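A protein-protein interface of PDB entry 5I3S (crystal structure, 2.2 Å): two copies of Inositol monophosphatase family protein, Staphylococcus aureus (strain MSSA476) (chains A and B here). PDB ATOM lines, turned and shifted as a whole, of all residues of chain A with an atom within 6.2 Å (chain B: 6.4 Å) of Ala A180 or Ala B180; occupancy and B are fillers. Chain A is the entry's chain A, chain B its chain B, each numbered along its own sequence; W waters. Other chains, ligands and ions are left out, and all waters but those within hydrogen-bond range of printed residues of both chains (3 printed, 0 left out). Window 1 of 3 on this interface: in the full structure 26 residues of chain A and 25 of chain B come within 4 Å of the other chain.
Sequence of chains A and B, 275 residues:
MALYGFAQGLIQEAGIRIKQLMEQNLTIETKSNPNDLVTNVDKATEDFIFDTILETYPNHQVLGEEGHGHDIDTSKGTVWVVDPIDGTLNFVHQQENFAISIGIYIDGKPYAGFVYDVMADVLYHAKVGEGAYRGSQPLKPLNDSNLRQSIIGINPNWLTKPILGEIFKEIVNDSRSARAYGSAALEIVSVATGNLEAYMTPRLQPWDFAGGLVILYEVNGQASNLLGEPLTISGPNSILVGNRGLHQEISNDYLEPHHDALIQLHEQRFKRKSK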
ATOM      1  N   ILE A 152      -1.243  31.999 -16.000  1.00  0.00           N
ATOM      2  CA  ILE A 152      -0.173  31.137 -16.403  1.00  0.00           C
ATOM      3  C   ILE A 152      -0.601  29.708 -16.431  1.00  0.00           C
ATOM      4  O   ILE A 152      -1.480  29.301 -15.690  1.00  0.00           O
ATOM      5  CB  ILE A 152       1.036  31.222 -15.442  1.00  0.00           C
ATOM      6  CG1 ILE A 152       0.727  30.639 -14.063  1.00  0.00           C
ATOM      7  CG2 ILE A 152       1.457  32.695 -15.297  1.00  0.00           C
ATOM      8  CD1 ILE A 152       1.903  30.693 -13.129  1.00  0.00           C
ATOM      9  N   GLY A 153       0.068  28.951 -17.284  1.00  0.00           N
ATOM     10  CA  GLY A 153      -0.142  27.557 -17.419  1.00  0.00           C
ATOM     11  C   GLY A 153       0.928  26.814 -16.653  1.00  0.00           C
ATOM     12  O   GLY A 153       2.123  27.040 -16.909  1.00  0.00           O
ATOM     13  N   ILE A 154       0.508  25.915 -15.753  1.00  0.00           N
ATOM     14  CA  ILE A 154       1.431  25.077 -15.023  1.00  0.00           C
ATOM     15  C   ILE A 154       0.679  23.920 -14.399  1.00  0.00           C
ATOM     16  O   ILE A 154      -0.332  24.137 -13.735  1.00  0.00           O
ATOM     17  CB  ILE A 154       2.204  25.878 -13.939  1.00  0.00           C
ATOM     18  CG1 ILE A 154       3.241  25.001 -13.248  1.00  0.00           C
ATOM     19  CG2 ILE A 154       1.282  26.490 -12.888  1.00  0.00           C
ATOM     20  CD1 ILE A 154       4.123  25.811 -12.299  1.00  0.00           C
ATOM     21  N   ASN A 155       1.143  22.696 -14.604  1.00  0.00           N
ATOM     22  CA  ASN A 155       0.414  21.523 -14.028  1.00  0.00           C
ATOM     23  C   ASN A 155       0.550  21.568 -12.509  1.00  0.00           C
ATOM     24  O   ASN A 155       1.636  21.788 -12.009  1.00  0.00           O
ATOM     25  CB  ASN A 155       0.887  20.200 -14.603  1.00  0.00           C
ATOM     26  CG  ASN A 155      -0.088  19.048 -14.371  1.00  0.00           C
ATOM     27  OD1 ASN A 155      -0.580  18.409 -15.310  1.00  0.00           O
ATOM     28  ND2 ASN A 155      -0.266  18.701 -13.171  1.00  0.00           N
ATOM     29  N   PRO A 156      -0.567  21.426 -11.774  1.00  0.00           N
ATOM     30  CA  PRO A 156      -0.466  21.319 -10.306  1.00  0.00           C
ATOM     31  C   PRO A 156       0.579  20.316  -9.753  1.00  0.00           C
ATOM     32  O   PRO A 156       1.144  20.532  -8.683  1.00  0.00           O
ATOM     33  CB  PRO A 156      -1.881  20.857  -9.910  1.00  0.00           C
ATOM     34  CG  PRO A 156      -2.783  21.463 -10.960  1.00  0.00           C
ATOM     35  CD  PRO A 156      -1.965  21.436 -12.235  1.00  0.00           C
ATOM     36  N   ALA A 178      -3.909  30.514 -12.229  1.00  0.00           N
ATOM     37  CA  ALA A 178      -3.239  29.445 -12.942  1.00  0.00           C
ATOM     38  C   ALA A 178      -4.217  28.445 -13.552  1.00  0.00           C
ATOM     39  O   ALA A 178      -5.259  28.143 -12.970  1.00  0.00           O
ATOM     40  CB  ALA A 178      -2.256  28.729 -12.014  1.00  0.00           C
ATOM     41  N   ARG A 179      -3.759  27.855 -14.662  1.00  0.00           N
ATOM     42  CA  ARG A 179      -4.503  26.953 -15.519  1.00  0.00           C
ATOM     43  C   ARG A 179      -3.583  25.794 -15.910  1.00  0.00           C
ATOM     44  O   ARG A 179      -2.377  25.905 -15.814  1.00  0.00           O
ATOM     45  CB  ARG A 179      -4.947  27.688 -16.801  1.00  0.00           C
ATOM     46  CG  ARG A 179      -5.770  28.936 -16.591  1.00  0.00           C
ATOM     47  CD  ARG A 179      -7.174  28.581 -16.076  1.00  0.00           C
ATOM     48  NE  ARG A 179      -8.009  29.765 -15.903  1.00  0.00           N
ATOM     49  CZ  ARG A 179      -8.113  30.491 -14.800  1.00  0.00           C
ATOM     50  NH1 ARG A 179      -7.441  30.184 -13.670  1.00  0.00           N
ATOM     51  NH2 ARG A 179      -8.937  31.531 -14.801  1.00  0.00           N
ATOM     52  N   ALA A 180      -4.168  24.688 -16.370  1.00  0.00           N
ATOM     53  CA  ALA A 180      -3.423  23.561 -16.923  1.00  0.00           C
ATOM     54  C   ALA A 180      -4.369  22.706 -17.733  1.00  0.00           C
ATOM     55  O   ALA A 180      -5.416  22.260 -17.229  1.00  0.00           O
ATOM     56  CB  ALA A 180      -2.810  22.708 -15.795  1.00  0.00           C
ATOM     57  N   TYR A 181      -3.991  22.460 -18.972  1.00  0.00           N
ATOM     58  CA  TYR A 181      -4.877  21.886 -19.980  1.00  0.00           C
ATOM     59  C   TYR A 181      -4.438  20.537 -20.444  1.00  0.00           C
ATOM     60  O   TYR A 181      -5.221  19.804 -21.018  1.00  0.00           O
ATOM     61  CB  TYR A 181      -4.993  22.850 -21.160  1.00  0.00           C
ATOM     62  CG  TYR A 181      -5.520  24.250 -20.782  1.00  0.00           C
ATOM     63  CD1 TYR A 181      -6.766  24.421 -20.168  1.00  0.00           C
ATOM     64  CD2 TYR A 181      -4.808  25.393 -21.098  1.00  0.00           C
ATOM     65  CE1 TYR A 181      -7.261  25.693 -19.850  1.00  0.00           C
ATOM     66  CE2 TYR A 181      -5.286  26.669 -20.783  1.00  0.00           C
ATOM     67  CZ  TYR A 181      -6.510  26.813 -20.143  1.00  0.00           C
ATOM     68  OH  TYR A 181      -6.962  28.074 -19.839  1.00  0.00           O
ATOM     69  N   GLY A 182      -3.174  20.194 -20.209  1.00  0.00           N
ATOM     70  CA  GLY A 182      -2.713  18.814 -20.367  1.00  0.00           C
ATOM     71  C   GLY A 182      -2.168  18.498 -21.755  1.00  0.00           C
ATOM     72  O   GLY A 182      -1.861  17.338 -22.003  1.00  0.00           O
ATOM     73  N   GLU A 187      -0.907  24.224 -25.152  1.00  0.00           N
ATOM     74  CA  GLU A 187      -0.584  25.279 -24.156  1.00  0.00           C
ATOM     75  C   GLU A 187       0.358  26.367 -24.708  1.00  0.00           C
ATOM     76  O   GLU A 187       0.219  27.541 -24.392  1.00  0.00           O
ATOM     77  CB  GLU A 187      -0.068  24.666 -22.845  1.00  0.00           C
ATOM     78  CG  GLU A 187      -1.214  24.072 -22.020  1.00  0.00           C
ATOM     79  CD  GLU A 187      -0.818  22.897 -21.159  1.00  0.00           C
ATOM     80  OE1 GLU A 187      -0.053  21.989 -21.606  1.00  0.00           O
ATOM     81  OE2 GLU A 187      -1.280  22.867 -20.026  1.00  0.00           O
ATOM     82  N   ILE B 152      -7.927  14.799 -12.143  1.00  0.00           N
ATOM     83  CA  ILE B 152      -8.631  15.643 -11.178  1.00  0.00           C
ATOM     84  C   ILE B 152      -8.477  17.101 -11.584  1.00  0.00           C
ATOM     85  O   ILE B 152      -7.500  17.432 -12.242  1.00  0.00           O
ATOM     86  CB  ILE B 152      -8.149  15.449  -9.728  1.00  0.00           C
ATOM     87  CG1 ILE B 152      -6.675  15.887  -9.531  1.00  0.00           C
ATOM     88  CG2 ILE B 152      -8.358  13.994  -9.317  1.00  0.00           C
ATOM     89  CD1 ILE B 152      -6.238  15.882  -8.083  1.00  0.00           C
ATOM     90  N   GLY B 153      -9.451  17.932 -11.197  1.00  0.00           N
ATOM     91  CA  GLY B 153      -9.432  19.348 -11.419  1.00  0.00           C
ATOM     92  C   GLY B 153      -9.170  20.035 -10.103  1.00  0.00           C
ATOM     93  O   GLY B 153      -9.868  19.796  -9.132  1.00  0.00           O
ATOM     94  N   ILE B 154      -8.103  20.827 -10.057  1.00  0.00           N
ATOM     95  CA  ILE B 154      -7.765  21.600  -8.879  1.00  0.00           C
ATOM     96  C   ILE B 154      -6.803  22.709  -9.318  1.00  0.00           C
ATOM     97  O   ILE B 154      -5.854  22.464 -10.004  1.00  0.00           O
ATOM     98  CB  ILE B 154      -7.121  20.707  -7.821  1.00  0.00           C
ATOM     99  CG1 ILE B 154      -6.802  21.519  -6.574  1.00  0.00           C
ATOM    100  CG2 ILE B 154      -5.846  20.023  -8.359  1.00  0.00           C
ATOM    101  CD1 ILE B 154      -6.080  20.677  -5.554  1.00  0.00           C
ATOM    102  N   ASN B 155      -7.021  23.918  -8.874  1.00  0.00           N
ATOM    103  CA  ASN B 155      -6.167  25.039  -9.278  1.00  0.00           C
ATOM    104  C   ASN B 155      -4.821  24.943  -8.554  1.00  0.00           C
ATOM    105  O   ASN B 155      -4.801  24.674  -7.376  1.00  0.00           O
ATOM    106  CB  ASN B 155      -6.896  26.320  -8.911  1.00  0.00           C
ATOM    107  CG  ASN B 155      -6.348  27.572  -9.601  1.00  0.00           C
ATOM    108  OD1 ASN B 155      -7.053  28.234 -10.338  1.00  0.00           O
ATOM    109  ND2 ASN B 155      -5.163  27.914  -9.309  1.00  0.00           N
ATOM    110  N   PRO B 156      -3.686  25.126  -9.256  1.00  0.00           N
ATOM    111  CA  PRO B 156      -2.386  25.186  -8.622  1.00  0.00           C
ATOM    112  C   PRO B 156      -2.281  26.086  -7.403  1.00  0.00           C
ATOM    113  O   PRO B 156      -1.606  25.773  -6.443  1.00  0.00           O
ATOM    114  CB  PRO B 156      -1.508  25.744  -9.752  1.00  0.00           C
ATOM    115  CG  PRO B 156      -2.074  25.065 -10.983  1.00  0.00           C
ATOM    116  CD  PRO B 156      -3.578  25.153 -10.725  1.00  0.00           C
ATOM    117  N   ALA B 178      -3.503  16.205 -13.189  1.00  0.00           N
ATOM    118  CA  ALA B 178      -4.357  17.299 -12.754  1.00  0.00           C
ATOM    119  C   ALA B 178      -4.536  18.312 -13.862  1.00  0.00           C
ATOM    120  O   ALA B 178      -3.697  18.417 -14.738  1.00  0.00           O
ATOM    121  CB  ALA B 178      -3.797  17.956 -11.529  1.00  0.00           C
ATOM    122  N   ARG B 179      -5.635  19.058 -13.780  1.00  0.00           N
ATOM    123  CA  ARG B 179      -6.058  20.074 -14.753  1.00  0.00           C
ATOM    124  C   ARG B 179      -6.730  21.210 -13.971  1.00  0.00           C
ATOM    125  O   ARG B 179      -7.214  20.976 -12.838  1.00  0.00           O
ATOM    126  CB  ARG B 179      -7.108  19.527 -15.713  1.00  0.00           C
ATOM    127  CG  ARG B 179      -6.726  18.345 -16.585  1.00  0.00           C
ATOM    128  CD  ARG B 179      -5.833  18.733 -17.727  1.00  0.00           C
ATOM    129  NE  ARG B 179      -5.461  17.536 -18.504  1.00  0.00           N
ATOM    130  CZ  ARG B 179      -4.489  16.666 -18.193  1.00  0.00           C
ATOM    131  NH1 ARG B 179      -3.719  16.810 -17.113  1.00  0.00           N
ATOM    132  NH2 ARG B 179      -4.270  15.628 -19.003  1.00  0.00           N
ATOM    133  N   ALA B 180      -6.795  22.408 -14.581  1.00  0.00           N
ATOM    134  CA  ALA B 180      -7.485  23.570 -14.023  1.00  0.00           C
ATOM    135  C   ALA B 180      -7.965  24.491 -15.149  1.00  0.00           C
ATOM    136  O   ALA B 180      -7.161  24.993 -15.937  1.00  0.00           O
ATOM    137  CB  ALA B 180      -6.563  24.347 -13.080  1.00  0.00           C
ATOM    138  N   TYR B 181      -9.286  24.717 -15.214  1.00  0.00           N
ATOM    139  CA  TYR B 181      -9.945  25.502 -16.288  1.00  0.00           C
ATOM    140  C   TYR B 181     -10.437  26.856 -15.840  1.00  0.00           C
ATOM    141  O   TYR B 181     -10.753  27.681 -16.674  1.00  0.00           O
ATOM    142  CB  TYR B 181     -11.105  24.713 -16.920  1.00  0.00           C
ATOM    143  CG  TYR B 181     -10.711  23.333 -17.339  1.00  0.00           C
ATOM    144  CD1 TYR B 181      -9.677  23.133 -18.228  1.00  0.00           C
ATOM    145  CD2 TYR B 181     -11.349  22.230 -16.864  1.00  0.00           C
ATOM    146  CE1 TYR B 181      -9.297  21.851 -18.617  1.00  0.00           C
ATOM    147  CE2 TYR B 181     -10.977  20.957 -17.252  1.00  0.00           C
ATOM    148  CZ  TYR B 181      -9.942  20.789 -18.121  1.00  0.00           C
ATOM    149  OH  TYR B 181      -9.579  19.548 -18.545  1.00  0.00           O
ATOM    150  N   GLY B 182     -10.539  27.097 -14.538  1.00  0.00           N
ATOM    151  CA  GLY B 182     -10.850  28.433 -14.044  1.00  0.00           C
ATOM    152  C   GLY B 182     -12.325  28.832 -14.067  1.00  0.00           C
ATOM    153  O   GLY B 182     -12.630  30.033 -13.912  1.00  0.00           O
ATOM    154  N   SER B 183     -13.241  27.863 -14.218  1.00  0.00           N
ATOM    155  CA  SER B 183     -14.705  28.095 -14.059  1.00  0.00           C
ATOM    156  C   SER B 183     -15.295  26.920 -13.345  1.00  0.00           C
ATOM    157  O   SER B 183     -15.407  25.824 -13.908  1.00  0.00           O
ATOM    158  CB  SER B 183     -15.410  28.331 -15.427  1.00  0.00           C
ATOM    159  OG  SER B 183     -16.841  28.365 -15.329  1.00  0.00           O
ATOM    160  N   GLU B 187     -16.259  23.119 -14.487  1.00  0.00           N
ATOM    161  CA  GLU B 187     -15.414  22.018 -13.930  1.00  0.00           C
ATOM    162  C   GLU B 187     -16.259  20.885 -13.325  1.00  0.00           C
ATOM    163  O   GLU B 187     -15.967  19.712 -13.481  1.00  0.00           O
ATOM    164  CB  GLU B 187     -14.340  22.536 -12.942  1.00  0.00           C
ATOM    165  CG  GLU B 187     -13.056  22.991 -13.664  1.00  0.00           C
ATOM    166  CD  GLU B 187     -12.244  24.034 -12.914  1.00  0.00           C
ATOM    167  OE1 GLU B 187     -12.846  24.900 -12.237  1.00  0.00           O
ATOM    168  OE2 GLU B 187     -11.011  24.010 -12.992  1.00  0.00           O
HETATM  169  O   HOH W   1      -7.940  19.625 -21.146  1.00  0.00           O
HETATM  170  O   HOH W   2     -11.795  32.518 -14.779  1.00  0.00           O
HETATM  171  O   HOH W   3      -3.089  14.589 -21.975  1.00  0.00           O
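The backbone carbonyl oxygen (O) of Tyr A181 sits at hydrogen-bond distance from the guanidinium group (NE) of Arg B179, 3.4 Å away. O of Ala A180 is in hydrogen-bond range of N of Ala B180. The side-chain amide oxygen (OD1) of Asn A155 sits close to the backbone carbonyl oxygen (O) of Ala B178 (3.2 Å). The backbone carbonyl oxygen (O) of Ala A178 sits close to the side-chain amide oxygen (OD1) of Asn B155 (3.2 Å).
Of the 11 printed residues of chain A, 8 touch a printed residue of chain B. Hydrophobic or aromatic side chains of chain A within 4 Å of the printed part of chain B: Pro A156, Ala A178 and Tyr A181. Of the 12 printed residues of chain B, 8 touch a printed residue of chain A.
Gly A153 touches none of the printed residues of chain B. Of the printed residues of chain B, Ile A154 touches Pro B156. Printed residues of chain B within 4 Å of Pro A156: Ile B154 (3.4 Å), Pro B156 (3.7 Å) and Ala B178 (3.7 Å). Of the printed residues of chain B, Tyr A181 touches Arg B179, Ala B180 and Tyr B181. Of the printed residues of chain B, Gly A182 touches Arg B179 (3.5 Å). Printed residues of chain A within 4 Å of Ala B180: Arg A179, Ala A180 and Tyr A181. Of the printed residues of chain A, Tyr B181 touches Arg A179 (3.5 Å) and Tyr A181 (3.7 Å). The nearest printed residue of chain B that does not touch Asn A155 is Pro B156 (4.6 Å).
Water W1 lies within hydrogen-bond range of O of Tyr A181 and OH of Tyr B181. Water W2 lies within hydrogen-bond range of O of Gly B182 (2.8 Å) and NH2 of Arg A179 (3.0 Å). Water W3 bridges the backbone carbonyl oxygen (O) of Gly A182 (3.0 Å) and the guanidinium group (NH2) of Arg B179 (3.4 Å).
Among the printed residues, merely in contact across the chains: Arg A179 with Ala B180 (3.3 Å), Ala A180 with Arg B179 (3.4 Å), Pro A156 with Ile B154 (3.4 Å), Ile A154 with Pro B156 (3.4 Å), Arg A179 with Gly B182 (3.5 Å), Arg A179 with Tyr B181 (3.5 Å), Gly A182 with Arg B179 (3.5 Å), Pro A156 with Pro B156 (3.7 Å), Pro A156 with Ala B178 (3.7 Å), Tyr A181 with Tyr B181 (3.7 Å), Ala A178 with Pro B156 (3.8 Å), Arg A179 with Asn B155 (3.9 Å), Asn A155 with Arg B179 (3.96 Å) and Tyr A181 with Ala B180 (3.98 Å).
Pro A156 touches its own counterpart, Pro B156. Arg A179 touches Tyr B181, and with the chains exchanged Tyr A181 touches Arg B179. Arg A179 touches Gly B182, and with the chains exchanged Gly A182 touches Arg B179. Ala A180 touches its own counterpart, Ala B180. 11 positions are printed for both chains.
The backbone NH (N) of Gly B182 sits at hydrogen-bond distance from the side-chain carboxylate (OE2) of Glu B187, at 3.5 Å. N of Ile B154 is in hydrogen-bond range of O of Arg B179 (2.9 Å). The backbone NH (N) of Ile A154 lies within hydrogen-bond range of the backbone carbonyl oxygen (O) of Arg A179, at 2.9 Å. N of Gly A182 is in hydrogen-bond range of OE2 of Glu A187 (3.3 Å). N of Tyr B181 lies within hydrogen-bond range of OE2 of Glu B187 (2.9 Å). O of Ile B152 sits at hydrogen-bond distance from N of Arg B179.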
